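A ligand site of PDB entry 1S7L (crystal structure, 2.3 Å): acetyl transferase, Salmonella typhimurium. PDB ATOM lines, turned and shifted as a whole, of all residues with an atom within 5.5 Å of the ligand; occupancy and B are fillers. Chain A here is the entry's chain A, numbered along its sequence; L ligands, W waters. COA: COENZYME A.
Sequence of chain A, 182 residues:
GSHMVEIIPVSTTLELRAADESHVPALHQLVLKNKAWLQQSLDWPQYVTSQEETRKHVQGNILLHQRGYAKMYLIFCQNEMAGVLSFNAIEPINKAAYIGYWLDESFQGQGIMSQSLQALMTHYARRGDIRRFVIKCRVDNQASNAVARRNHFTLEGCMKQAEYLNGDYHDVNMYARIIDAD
The side-chain sulfur of Cys 137 is bonded to a sulfur (S1P) of the ligand (2.3 Å).
The guanidinium group (NH2) of Arg 150 is in salt-bridge range of an oxygen (O8A) of the ligand (2.6 Å).
The side-chain amide nitrogen of Asn 141 sits at hydrogen-bond distance from an oxygen (O5P) of the ligand (2.7 Å).
The backbone NH (N) of Leu 103 lies within hydrogen-bond range of an oxygen (O9P) of the ligand (2.8 Å).
The backbone NH of Ser 114 lies within hydrogen-bond range of an oxygen (O1A) of the ligand (2.8 Å).
An oxygen (O1A) of the ligand sits at hydrogen-bond distance from the side-chain hydroxyl (OG) of Ser 114, at 2.9 Å.
An oxygen (O2A) of the ligand is in hydrogen-bond range of the backbone NH (N) of Met 113, at 2.8 Å.
The backbone NH (N) of Gly 109 lies within hydrogen-bond range of an oxygen (O4A) of the ligand, at 2.9 Å.
O5B of the ligand is in hydrogen-bond range of N of Gly 111.
The backbone carbonyl oxygen (O) of Tyr 101 lies within hydrogen-bond range of a nitrogen (N4P) of the ligand, 2.9 Å away.
The backbone NH (N) of Ile 112 lies within hydrogen-bond range of an oxygen (O2A) of the ligand.
An oxygen (O4B) of the ligand is in hydrogen-bond range of the backbone NH (N) of Gln 110, 3.2 Å away.
O5P of the ligand lies within hydrogen-bond range of OG of Ser 41, at 3.3 Å.
The side-chain sulfur of Cys 137 lies within hydrogen-bond range of the side-chain amide nitrogen of Asn 141 (3.3 Å).
NE of Arg 150 is in hydrogen-bond range of OG of Ser 114.
OD1 of Asn 141 lies within hydrogen-bond range of N of Ser 144, at 3.0 Å.
NE2 of Gln 108 sits at hydrogen-bond distance from O of Leu 103, at 3.1 Å.
NE2 of Gln 115 lies close to O of Gly 111.
The side-chain hydroxyl (OH) of Tyr 101 lies within hydrogen-bond range of the side-chain hydroxyl (OG) of Ser 144 (2.7 Å).
Residues that only touch the ligand: Ala 146 (3.1 Å), Gln 108 (3.2 Å), Trp 102 (3.3 Å), Ser 144 (3.4 Å), Trp 37 (3.4 Å), Ala 143 (3.5 Å), Val 147 (3.9 Å), Lys 136 (3.9 Å) and Leu 38 (3.98 Å).
Hydrophobic or aromatic side chains within 4 Å of the ligand: Trp 37, Leu 38, Tyr 101, Trp 102, Leu 103, Met 113, Ala 143, Ala 146 and Val 147.
Water W2 bridges O5A of the ligand (2.5 Å) and O of Ala 143 (2.8 Å).
Water W1 lies within hydrogen-bond range of the side-chain amide oxygen of Gln 108 (2.5 Å) and an oxygen (OAP) of the ligand (2.8 Å).
Water W3 bridges the side-chain amide oxygen (OD1) of Asn 141 (2.8 Å) and an oxygen (OAP) of the ligand (3.0 Å).
Water W4 lies within hydrogen-bond range of the backbone carbonyl oxygen of Lys 136 and the backbone carbonyl oxygen of Ile 99.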
ATOM      1  N   TRP A  37     -17.230   2.781 -17.149  1.00  0.00           N
ATOM      2  CA  TRP A  37     -18.501   3.463 -17.316  1.00  0.00           C
ATOM      3  C   TRP A  37     -19.267   3.658 -16.009  1.00  0.00           C
ATOM      4  O   TRP A  37     -20.031   4.612 -15.899  1.00  0.00           O
ATOM      5  CB  TRP A  37     -19.343   2.757 -18.391  1.00  0.00           C
ATOM      6  CG  TRP A  37     -19.829   1.404 -18.015  1.00  0.00           C
ATOM      7  CD1 TRP A  37     -19.210   0.200 -18.212  1.00  0.00           C
ATOM      8  CD2 TRP A  37     -21.019   1.123 -17.283  1.00  0.00           C
ATOM      9  NE1 TRP A  37     -19.928  -0.807 -17.623  1.00  0.00           N
ATOM     10  CE2 TRP A  37     -21.055  -0.270 -17.040  1.00  0.00           C
ATOM     11  CE3 TRP A  37     -22.057   1.912 -16.794  1.00  0.00           C
ATOM     12  CZ2 TRP A  37     -22.081  -0.881 -16.336  1.00  0.00           C
ATOM     13  CZ3 TRP A  37     -23.087   1.289 -16.082  1.00  0.00           C
ATOM     14  CH2 TRP A  37     -23.075  -0.089 -15.860  1.00  0.00           C
ATOM     15  N   LEU A  38     -19.043   2.815 -15.004  1.00  0.00           N
ATOM     16  CA  LEU A  38     -19.709   2.956 -13.687  1.00  0.00           C
ATOM     17  C   LEU A  38     -19.337   4.290 -13.035  1.00  0.00           C
ATOM     18  O   LEU A  38     -20.131   4.897 -12.352  1.00  0.00           O
ATOM     19  CB  LEU A  38     -19.299   1.853 -12.713  1.00  0.00           C
ATOM     20  CG  LEU A  38     -19.980   0.495 -12.874  1.00  0.00           C
ATOM     21  CD1 LEU A  38     -19.225  -0.519 -12.014  1.00  0.00           C
ATOM     22  CD2 LEU A  38     -21.479   0.557 -12.538  1.00  0.00           C
ATOM     23  N   SER A  41     -21.585   7.506 -12.697  1.00  0.00           N
ATOM     24  CA  SER A  41     -22.690   7.732 -11.764  1.00  0.00           C
ATOM     25  C   SER A  41     -22.443   7.193 -10.337  1.00  0.00           C
ATOM     26  O   SER A  41     -23.249   7.443  -9.427  1.00  0.00           O
ATOM     27  CB  SER A  41     -24.011   7.219 -12.361  1.00  0.00           C
ATOM     28  OG  SER A  41     -23.893   5.871 -12.708  1.00  0.00           O
ATOM     29  N   LEU A  42     -21.331   6.495 -10.143  1.00  0.00           N
ATOM     30  CA  LEU A  42     -20.970   5.979  -8.821  1.00  0.00           C
ATOM     31  C   LEU A  42     -19.615   6.539  -8.453  1.00  0.00           C
ATOM     32  O   LEU A  42     -18.796   6.803  -9.329  1.00  0.00           O
ATOM     33  CB  LEU A  42     -20.906   4.458  -8.796  1.00  0.00           C
ATOM     34  CG  LEU A  42     -22.224   3.739  -9.107  1.00  0.00           C
ATOM     35  CD1 LEU A  42     -22.152   2.357  -8.506  1.00  0.00           C
ATOM     36  CD2 LEU A  42     -23.429   4.511  -8.570  1.00  0.00           C
ATOM     37  N   ILE A  99     -31.576   2.963  -1.689  1.00  0.00           N
ATOM     38  CA  ILE A  99     -31.179   1.935  -2.644  1.00  0.00           C
ATOM     39  C   ILE A  99     -29.981   2.272  -3.537  1.00  0.00           C
ATOM     40  O   ILE A  99     -29.827   3.392  -3.954  1.00  0.00           O
ATOM     41  CB  ILE A  99     -32.362   1.564  -3.565  1.00  0.00           C
ATOM     42  CG1 ILE A  99     -33.414   0.844  -2.732  1.00  0.00           C
ATOM     43  CG2 ILE A  99     -31.906   0.712  -4.767  1.00  0.00           C
ATOM     44  CD1 ILE A  99     -34.862   1.123  -3.244  1.00  0.00           C
ATOM     45  N   GLY A 100     -29.140   1.277  -3.788  1.00  0.00           N
ATOM     46  CA  GLY A 100     -28.073   1.427  -4.722  1.00  0.00           C
ATOM     47  C   GLY A 100     -28.100   0.123  -5.577  1.00  0.00           C
ATOM     48  O   GLY A 100     -28.495  -0.973  -5.075  1.00  0.00           O
ATOM     49  N   TYR A 101     -27.731   0.220  -6.862  1.00  0.00           N
ATOM     50  CA  TYR A 101     -27.640  -0.963  -7.755  1.00  0.00           C
ATOM     51  C   TYR A 101     -26.838  -0.627  -9.006  1.00  0.00           C
ATOM     52  O   TYR A 101     -26.680   0.545  -9.357  1.00  0.00           O
ATOM     53  CB  TYR A 101     -29.031  -1.480  -8.235  1.00  0.00           C
ATOM     54  CG  TYR A 101     -29.999  -0.410  -8.765  1.00  0.00           C
ATOM     55  CD1 TYR A 101     -29.655   0.412  -9.855  1.00  0.00           C
ATOM     56  CD2 TYR A 101     -31.206  -0.148  -8.105  1.00  0.00           C
ATOM     57  CE1 TYR A 101     -30.473   1.473 -10.283  1.00  0.00           C
ATOM     58  CE2 TYR A 101     -32.046   0.931  -8.517  1.00  0.00           C
ATOM     59  CZ  TYR A 101     -31.672   1.733  -9.635  1.00  0.00           C
ATOM     60  OH  TYR A 101     -32.521   2.752 -10.062  1.00  0.00           O
ATOM     61  N   TRP A 102     -26.308  -1.671  -9.642  1.00  0.00           N
ATOM     62  CA  TRP A 102     -25.661  -1.512 -10.920  1.00  0.00           C
ATOM     63  C   TRP A 102     -25.663  -2.861 -11.539  1.00  0.00           C
ATOM     64  O   TRP A 102     -25.697  -3.869 -10.831  1.00  0.00           O
ATOM     65  CB  TRP A 102     -24.225  -0.950 -10.836  1.00  0.00           C
ATOM     66  CG  TRP A 102     -23.196  -1.776 -10.058  1.00  0.00           C
ATOM     67  CD1 TRP A 102     -22.902  -1.673  -8.733  1.00  0.00           C
ATOM     68  CD2 TRP A 102     -22.274  -2.748 -10.587  1.00  0.00           C
ATOM     69  NE1 TRP A 102     -21.868  -2.527  -8.388  1.00  0.00           N
ATOM     70  CE2 TRP A 102     -21.455  -3.192  -9.506  1.00  0.00           C
ATOM     71  CE3 TRP A 102     -22.048  -3.291 -11.868  1.00  0.00           C
ATOM     72  CZ2 TRP A 102     -20.425  -4.132  -9.671  1.00  0.00           C
ATOM     73  CZ3 TRP A 102     -21.010  -4.233 -12.044  1.00  0.00           C
ATOM     74  CH2 TRP A 102     -20.207  -4.651 -10.935  1.00  0.00           C
ATOM     75  N   LEU A 103     -25.650  -2.879 -12.873  1.00  0.00           N
ATOM     76  CA  LEU A 103     -25.654  -4.145 -13.646  1.00  0.00           C
ATOM     77  C   LEU A 103     -24.482  -4.256 -14.626  1.00  0.00           C
ATOM     78  O   LEU A 103     -24.198  -3.284 -15.288  1.00  0.00           O
ATOM     79  CB  LEU A 103     -26.916  -4.241 -14.488  1.00  0.00           C
ATOM     80  CG  LEU A 103     -28.173  -5.036 -14.066  1.00  0.00           C
ATOM     81  CD1 LEU A 103     -29.205  -5.061 -15.279  1.00  0.00           C
ATOM     82  CD2 LEU A 103     -27.772  -6.479 -13.587  1.00  0.00           C
ATOM     83  N   PHE A 107     -25.480  -7.620 -19.150  1.00  0.00           N
ATOM     84  CA  PHE A 107     -26.742  -8.118 -18.606  1.00  0.00           C
ATOM     85  C   PHE A 107     -27.846  -7.030 -18.666  1.00  0.00           C
ATOM     86  O   PHE A 107     -28.919  -7.225 -18.168  1.00  0.00           O
ATOM     87  CB  PHE A 107     -26.556  -8.635 -17.139  1.00  0.00           C
ATOM     88  CG  PHE A 107     -25.877  -9.991 -17.060  1.00  0.00           C
ATOM     89  CD1 PHE A 107     -24.493 -10.089 -17.034  1.00  0.00           C
ATOM     90  CD2 PHE A 107     -26.624 -11.182 -17.099  1.00  0.00           C
ATOM     91  CE1 PHE A 107     -23.844 -11.350 -17.052  1.00  0.00           C
ATOM     92  CE2 PHE A 107     -26.002 -12.449 -17.127  1.00  0.00           C
ATOM     93  CZ  PHE A 107     -24.601 -12.534 -17.099  1.00  0.00           C
ATOM     94  N   GLN A 108     -27.555  -5.884 -19.251  1.00  0.00           N
ATOM     95  CA  GLN A 108     -28.547  -4.835 -19.391  1.00  0.00           C
ATOM     96  C   GLN A 108     -29.616  -5.000 -20.514  1.00  0.00           C
ATOM     97  O   GLN A 108     -29.461  -5.842 -21.434  1.00  0.00           O
ATOM     98  CB  GLN A 108     -27.825  -3.511 -19.574  1.00  0.00           C
ATOM     99  CG  GLN A 108     -27.081  -3.122 -18.348  1.00  0.00           C
ATOM    100  CD  GLN A 108     -26.347  -1.812 -18.494  1.00  0.00           C
ATOM    101  OE1 GLN A 108     -26.595  -1.035 -19.463  1.00  0.00           O
ATOM    102  NE2 GLN A 108     -25.442  -1.527 -17.525  1.00  0.00           N
ATOM    103  N   GLY A 109     -30.676  -4.208 -20.438  1.00  0.00           N
ATOM    104  CA  GLY A 109     -31.672  -4.284 -21.459  1.00  0.00           C
ATOM    105  C   GLY A 109     -32.555  -5.525 -21.378  1.00  0.00           C
ATOM    106  O   GLY A 109     -33.239  -5.800 -22.339  1.00  0.00           O
ATOM    107  N   GLN A 110     -32.571  -6.238 -20.251  1.00  0.00           N
ATOM    108  CA  GLN A 110     -33.411  -7.407 -20.132  1.00  0.00           C
ATOM    109  C   GLN A 110     -34.415  -7.337 -18.998  1.00  0.00           C
ATOM    110  O   GLN A 110     -35.033  -8.363 -18.649  1.00  0.00           O
ATOM    111  CB  GLN A 110     -32.519  -8.650 -19.923  1.00  0.00           C
ATOM    112  CG  GLN A 110     -31.672  -9.003 -21.122  1.00  0.00           C
ATOM    113  CD  GLN A 110     -30.622 -10.059 -20.781  1.00  0.00           C
ATOM    114  OE1 GLN A 110     -30.961 -11.205 -20.390  1.00  0.00           O
ATOM    115  NE2 GLN A 110     -29.327  -9.706 -20.920  1.00  0.00           N
ATOM    116  N   GLY A 111     -34.608  -6.136 -18.446  1.00  0.00           N
ATOM    117  CA  GLY A 111     -35.492  -5.958 -17.301  1.00  0.00           C
ATOM    118  C   GLY A 111     -34.979  -6.680 -16.025  1.00  0.00           C
ATOM    119  O   GLY A 111     -35.740  -6.877 -15.072  1.00  0.00           O
ATOM    120  N   ILE A 112     -33.712  -7.096 -16.004  1.00  0.00           N
ATOM    121  CA  ILE A 112     -33.179  -7.783 -14.823  1.00  0.00           C
ATOM    122  C   ILE A 112     -33.190  -6.947 -13.552  1.00  0.00           C
ATOM    123  O   ILE A 112     -33.664  -7.380 -12.515  1.00  0.00           O
ATOM    124  CB  ILE A 112     -31.757  -8.354 -15.072  1.00  0.00           C
ATOM    125  CG1 ILE A 112     -31.866  -9.586 -16.006  1.00  0.00           C
ATOM    126  CG2 ILE A 112     -31.064  -8.679 -13.775  1.00  0.00           C
ATOM    127  CD1 ILE A 112     -30.617 -10.251 -16.403  1.00  0.00           C
ATOM    128  N   MET A 113     -32.711  -5.728 -13.632  1.00  0.00           N
ATOM    129  CA  MET A 113     -32.736  -4.891 -12.432  1.00  0.00           C
ATOM    130  C   MET A 113     -34.175  -4.480 -11.996  1.00  0.00           C
ATOM    131  O   MET A 113     -34.529  -4.419 -10.784  1.00  0.00           O
ATOM    132  CB  MET A 113     -31.854  -3.639 -12.655  1.00  0.00           C
ATOM    133  CG  MET A 113     -31.722  -2.786 -11.378  1.00  0.00           C
ATOM    134  SD  MET A 113     -30.954  -3.694 -10.013  1.00  0.00           S
ATOM    135  CE  MET A 113     -29.363  -3.899 -10.684  1.00  0.00           C
ATOM    136  N   SER A 114     -35.005  -4.167 -12.987  1.00  0.00           N
ATOM    137  CA  SER A 114     -36.394  -3.810 -12.683  1.00  0.00           C
ATOM    138  C   SER A 114     -37.019  -4.933 -11.852  1.00  0.00           C
ATOM    139  O   SER A 114     -37.629  -4.675 -10.818  1.00  0.00           O
ATOM    140  CB  SER A 114     -37.217  -3.675 -13.961  1.00  0.00           C
ATOM    141  OG  SER A 114     -36.895  -2.523 -14.691  1.00  0.00           O
ATOM    142  N   GLN A 115     -36.896  -6.175 -12.316  1.00  0.00           N
ATOM    143  CA  GLN A 115     -37.525  -7.280 -11.604  1.00  0.00           C
ATOM    144  C   GLN A 115     -36.886  -7.560 -10.229  1.00  0.00           C
ATOM    145  O   GLN A 115     -37.583  -7.967  -9.305  1.00  0.00           O
ATOM    146  CB  GLN A 115     -37.444  -8.598 -12.387  1.00  0.00           C
ATOM    147  CG  GLN A 115     -37.778  -8.487 -13.808  1.00  0.00           C
ATOM    148  CD  GLN A 115     -37.647  -9.825 -14.516  1.00  0.00           C
ATOM    149  OE1 GLN A 115     -38.402 -10.749 -14.204  1.00  0.00           O
ATOM    150  NE2 GLN A 115     -36.708  -9.936 -15.481  1.00  0.00           N
ATOM    151  N   ILE A 135     -34.440   6.273  -3.951  1.00  0.00           N
ATOM    152  CA  ILE A 135     -33.383   6.194  -4.966  1.00  0.00           C
ATOM    153  C   ILE A 135     -32.902   7.645  -5.307  1.00  0.00           C
ATOM    154  O   ILE A 135     -33.683   8.506  -5.698  1.00  0.00           O
ATOM    155  CB  ILE A 135     -33.869   5.506  -6.269  1.00  0.00           C
ATOM    156  CG1 ILE A 135     -34.273   4.050  -5.977  1.00  0.00           C
ATOM    157  CG2 ILE A 135     -32.757   5.510  -7.318  1.00  0.00           C
ATOM    158  CD1 ILE A 135     -34.895   3.317  -7.178  1.00  0.00           C
ATOM    159  N   LYS A 136     -31.628   7.902  -5.086  1.00  0.00           N
ATOM    160  CA  LYS A 136     -30.970   9.179  -5.370  1.00  0.00           C
ATOM    161  C   LYS A 136     -29.940   8.808  -6.452  1.00  0.00           C
ATOM    162  O   LYS A 136     -29.136   7.874  -6.289  1.00  0.00           O
ATOM    163  CB  LYS A 136     -30.132   9.694  -4.200  1.00  0.00           C
ATOM    164  CG  LYS A 136     -30.851   9.970  -2.905  1.00  0.00           C
ATOM    165  CD  LYS A 136     -29.875  10.053  -1.715  1.00  0.00           C
ATOM    166  CE  LYS A 136     -28.904  11.211  -1.834  1.00  0.00           C
ATOM    167  NZ  LYS A 136     -28.023  11.330  -0.639  1.00  0.00           N
ATOM    168  N   CYS A 137     -29.934   9.571  -7.524  1.00  0.00           N
ATOM    169  CA  CYS A 137     -29.020   9.346  -8.631  1.00  0.00           C
ATOM    170  C   CYS A 137     -29.035  10.620  -9.483  1.00  0.00           C
ATOM    171  O   CYS A 137     -30.027  11.413  -9.463  1.00  0.00           O
ATOM    172  CB  CYS A 137     -29.506   8.118  -9.435  1.00  0.00           C
ATOM    173  SG  CYS A 137     -28.308   7.567 -10.659  1.00  0.00           S
ATOM    174  N   ARG A 138     -27.951  10.883 -10.202  1.00  0.00           N
ATOM    175  CA  ARG A 138     -27.926  12.065 -11.091  1.00  0.00           C
ATOM    176  C   ARG A 138     -29.222  12.194 -11.840  1.00  0.00           C
ATOM    177  O   ARG A 138     -29.776  11.211 -12.314  1.00  0.00           O
ATOM    178  CB  ARG A 138     -26.857  11.928 -12.134  1.00  0.00           C
ATOM    179  CG  ARG A 138     -25.507  12.186 -11.638  1.00  0.00           C
ATOM    180  CD  ARG A 138     -24.484  11.652 -12.648  1.00  0.00           C
ATOM    181  NE  ARG A 138     -24.532  12.261 -13.976  1.00  0.00           N
ATOM    182  CZ  ARG A 138     -23.441  12.461 -14.733  1.00  0.00           C
ATOM    183  NH1 ARG A 138     -22.237  12.113 -14.275  1.00  0.00           N
ATOM    184  NH2 ARG A 138     -23.571  13.016 -15.945  1.00  0.00           N
ATOM    185  N   ASN A 141     -29.272  10.338 -15.361  1.00  0.00           N
ATOM    186  CA  ASN A 141     -29.136   8.881 -15.521  1.00  0.00           C
ATOM    187  C   ASN A 141     -30.552   8.348 -15.921  1.00  0.00           C
ATOM    188  O   ASN A 141     -31.364   7.954 -15.047  1.00  0.00           O
ATOM    189  CB  ASN A 141     -28.720   8.267 -14.199  1.00  0.00           C
ATOM    190  CG  ASN A 141     -28.322   6.829 -14.330  1.00  0.00           C
ATOM    191  OD1 ASN A 141     -28.934   6.061 -15.106  1.00  0.00           O
ATOM    192  ND2 ASN A 141     -27.304   6.441 -13.579  1.00  0.00           N
ATOM    193  N   ALA A 143     -31.528   5.593 -17.524  1.00  0.00           N
ATOM    194  CA  ALA A 143     -31.723   4.165 -17.321  1.00  0.00           C
ATOM    195  C   ALA A 143     -32.177   3.887 -15.861  1.00  0.00           C
ATOM    196  O   ALA A 143     -33.088   3.099 -15.636  1.00  0.00           O
ATOM    197  CB  ALA A 143     -30.410   3.387 -17.629  1.00  0.00           C
ATOM    198  N   SER A 144     -31.546   4.540 -14.879  1.00  0.00           N
ATOM    199  CA  SER A 144     -31.933   4.336 -13.486  1.00  0.00           C
ATOM    200  C   SER A 144     -33.290   4.959 -13.259  1.00  0.00           C
ATOM    201  O   SER A 144     -34.113   4.410 -12.582  1.00  0.00           O
ATOM    202  CB  SER A 144     -30.913   4.942 -12.522  1.00  0.00           C
ATOM    203  OG  SER A 144     -31.385   4.904 -11.162  1.00  0.00           O
ATOM    204  N   ALA A 146     -35.729   5.177 -15.317  1.00  0.00           N
ATOM    205  CA  ALA A 146     -36.726   4.231 -15.855  1.00  0.00           C
ATOM    206  C   ALA A 146     -36.950   3.058 -14.857  1.00  0.00           C
ATOM    207  O   ALA A 146     -38.052   2.639 -14.665  1.00  0.00           O
ATOM    208  CB  ALA A 146     -36.255   3.697 -17.222  1.00  0.00           C
ATOM    209  N   VAL A 147     -35.917   2.520 -14.240  1.00  0.00           N
ATOM    210  CA  VAL A 147     -36.102   1.452 -13.237  1.00  0.00           C
ATOM    211  C   VAL A 147     -36.975   1.972 -12.054  1.00  0.00           C
ATOM    212  O   VAL A 147     -37.823   1.241 -11.528  1.00  0.00           O
ATOM    213  CB  VAL A 147     -34.739   1.021 -12.625  1.00  0.00           C
ATOM    214  CG1 VAL A 147     -34.934  -0.002 -11.495  1.00  0.00           C
ATOM    215  CG2 VAL A 147     -33.854   0.482 -13.700  1.00  0.00           C
ATOM    216  N   ARG A 150     -40.650   2.526 -13.264  1.00  0.00           N
ATOM    217  CA  ARG A 150     -41.352   1.281 -13.518  1.00  0.00           C
ATOM    218  C   ARG A 150     -41.673   0.660 -12.158  1.00  0.00           C
ATOM    219  O   ARG A 150     -42.660  -0.029 -12.047  1.00  0.00           O
ATOM    220  CB  ARG A 150     -40.556   0.305 -14.393  1.00  0.00           C
ATOM    221  CG  ARG A 150     -41.043  -1.131 -14.350  1.00  0.00           C
ATOM    222  CD  ARG A 150     -40.660  -1.941 -15.619  1.00  0.00           C
ATOM    223  NE  ARG A 150     -39.343  -1.551 -15.967  1.00  0.00           N
ATOM    224  CZ  ARG A 150     -38.947  -0.905 -17.056  1.00  0.00           C
ATOM    225  NH1 ARG A 150     -39.737  -0.554 -18.049  1.00  0.00           N
ATOM    226  NH2 ARG A 150     -37.686  -0.548 -17.087  1.00  0.00           N
HETATM  227  N1A COA L   1     -39.177  -5.517 -18.054  1.00  0.00           N
HETATM  228  C2A COA L   1     -38.516  -4.335 -18.032  1.00  0.00           C
HETATM  229  N3A COA L   1     -37.640  -3.909 -18.890  1.00  0.00           N
HETATM  230  C4A COA L   1     -37.371  -4.747 -19.983  1.00  0.00           C
HETATM  231  C5A COA L   1     -38.007  -5.996 -20.118  1.00  0.00           C
HETATM  232  C6A COA L   1     -38.948  -6.371 -19.086  1.00  0.00           C
HETATM  233  N6A COA L   1     -39.554  -7.581 -19.161  1.00  0.00           N
HETATM  234  N7A COA L   1     -37.612  -6.650 -21.243  1.00  0.00           N
HETATM  235  C8A COA L   1     -36.723  -5.882 -21.824  1.00  0.00           C
HETATM  236  N9A COA L   1     -36.541  -4.746 -21.087  1.00  0.00           N
HETATM  237  C1B COA L   1     -35.530  -3.693 -21.382  1.00  0.00           C
HETATM  238  C2B COA L   1     -35.897  -2.277 -21.674  1.00  0.00           C
HETATM  239  O2B COA L   1     -35.446  -2.001 -22.969  1.00  0.00           O
HETATM  240  C3B COA L   1     -35.056  -1.377 -20.734  1.00  0.00           C
HETATM  241  O3B COA L   1     -35.958  -0.672 -20.090  1.00  0.00           O
HETATM  242  P3B COA L   1     -36.083   0.855 -19.808  1.00  0.00           P
HETATM  243  O7A COA L   1     -35.191   1.650 -20.611  1.00  0.00           O
HETATM  244  O8A COA L   1     -35.839   0.872 -18.296  1.00  0.00           O
HETATM  245  O9A COA L   1     -37.469   1.097 -20.200  1.00  0.00           O
HETATM  246  C4B COA L   1     -34.369  -2.438 -19.819  1.00  0.00           C
HETATM  247  O4B COA L   1     -34.538  -3.693 -20.371  1.00  0.00           O
HETATM  248  C5B COA L   1     -34.645  -2.600 -18.360  1.00  0.00           C
HETATM  249  O5B COA L   1     -33.605  -3.482 -17.857  1.00  0.00           O
HETATM  250  P1A COA L   1     -33.049  -3.283 -16.337  1.00  0.00           P
HETATM  251  O1A COA L   1     -34.168  -3.016 -15.402  1.00  0.00           O
HETATM  252  O2A COA L   1     -32.233  -4.436 -16.099  1.00  0.00           O
HETATM  253  O3A COA L   1     -32.259  -1.951 -16.357  1.00  0.00           O
HETATM  254  P2A COA L   1     -31.024  -1.522 -17.280  1.00  0.00           P
HETATM  255  O4A COA L   1     -30.449  -2.628 -17.998  1.00  0.00           O
HETATM  256  O5A COA L   1     -31.447  -0.347 -18.089  1.00  0.00           O
HETATM  257  O6A COA L   1     -29.910  -0.947 -16.341  1.00  0.00           O
HETATM  258  CBP COA L   1     -29.069   0.284 -14.461  1.00  0.00           C
HETATM  259  CCP COA L   1     -30.243   0.068 -15.425  1.00  0.00           C
HETATM  260  CDP COA L   1     -29.404   1.560 -13.673  1.00  0.00           C
HETATM  261  CEP COA L   1     -29.031  -0.975 -13.525  1.00  0.00           C
HETATM  262  CAP COA L   1     -27.709   0.463 -15.232  1.00  0.00           C
HETATM  263  OAP COA L   1     -27.800   1.524 -16.135  1.00  0.00           O
HETATM  264  C9P COA L   1     -26.459   0.641 -14.367  1.00  0.00           C
HETATM  265  O9P COA L   1     -25.920  -0.301 -13.929  1.00  0.00           O
HETATM  266  N8P COA L   1     -26.032   1.951 -14.181  1.00  0.00           N
HETATM  267  C7P COA L   1     -24.964   2.350 -13.223  1.00  0.00           C
HETATM  268  C6P COA L   1     -25.388   2.317 -11.741  1.00  0.00           C
HETATM  269  C5P COA L   1     -26.430   3.352 -11.466  1.00  0.00           C
HETATM  270  O5P COA L   1     -26.713   4.155 -12.270  1.00  0.00           O
HETATM  271  N4P COA L   1     -27.108   3.251 -10.317  1.00  0.00           N
HETATM  272  C3P COA L   1     -28.249   4.138 -10.023  1.00  0.00           C
HETATM  273  C2P COA L   1     -28.012   4.970  -8.790  1.00  0.00           C
HETATM  274  S1P COA L   1     -26.990   6.415  -9.220  1.00  0.00           S
HETATM  275  O   HOH W   1     -28.234   0.634 -18.709  1.00  0.00           O
HETATM  276  O   HOH W   2     -33.359   1.156 -17.651  1.00  0.00           O
HETATM  277  O   HOH W   3     -26.943   4.354 -15.977  1.00  0.00           O
HETATM  278  O   HOH W   4     -28.559   5.442  -5.453  1.00  0.00           O
HETATM  279  O   HOH W   5     -33.666   0.408 -23.048  1.00  0.00           O
HETATM  280  O   HOH W   6     -31.513  -6.397 -17.761  1.00  0.00           O
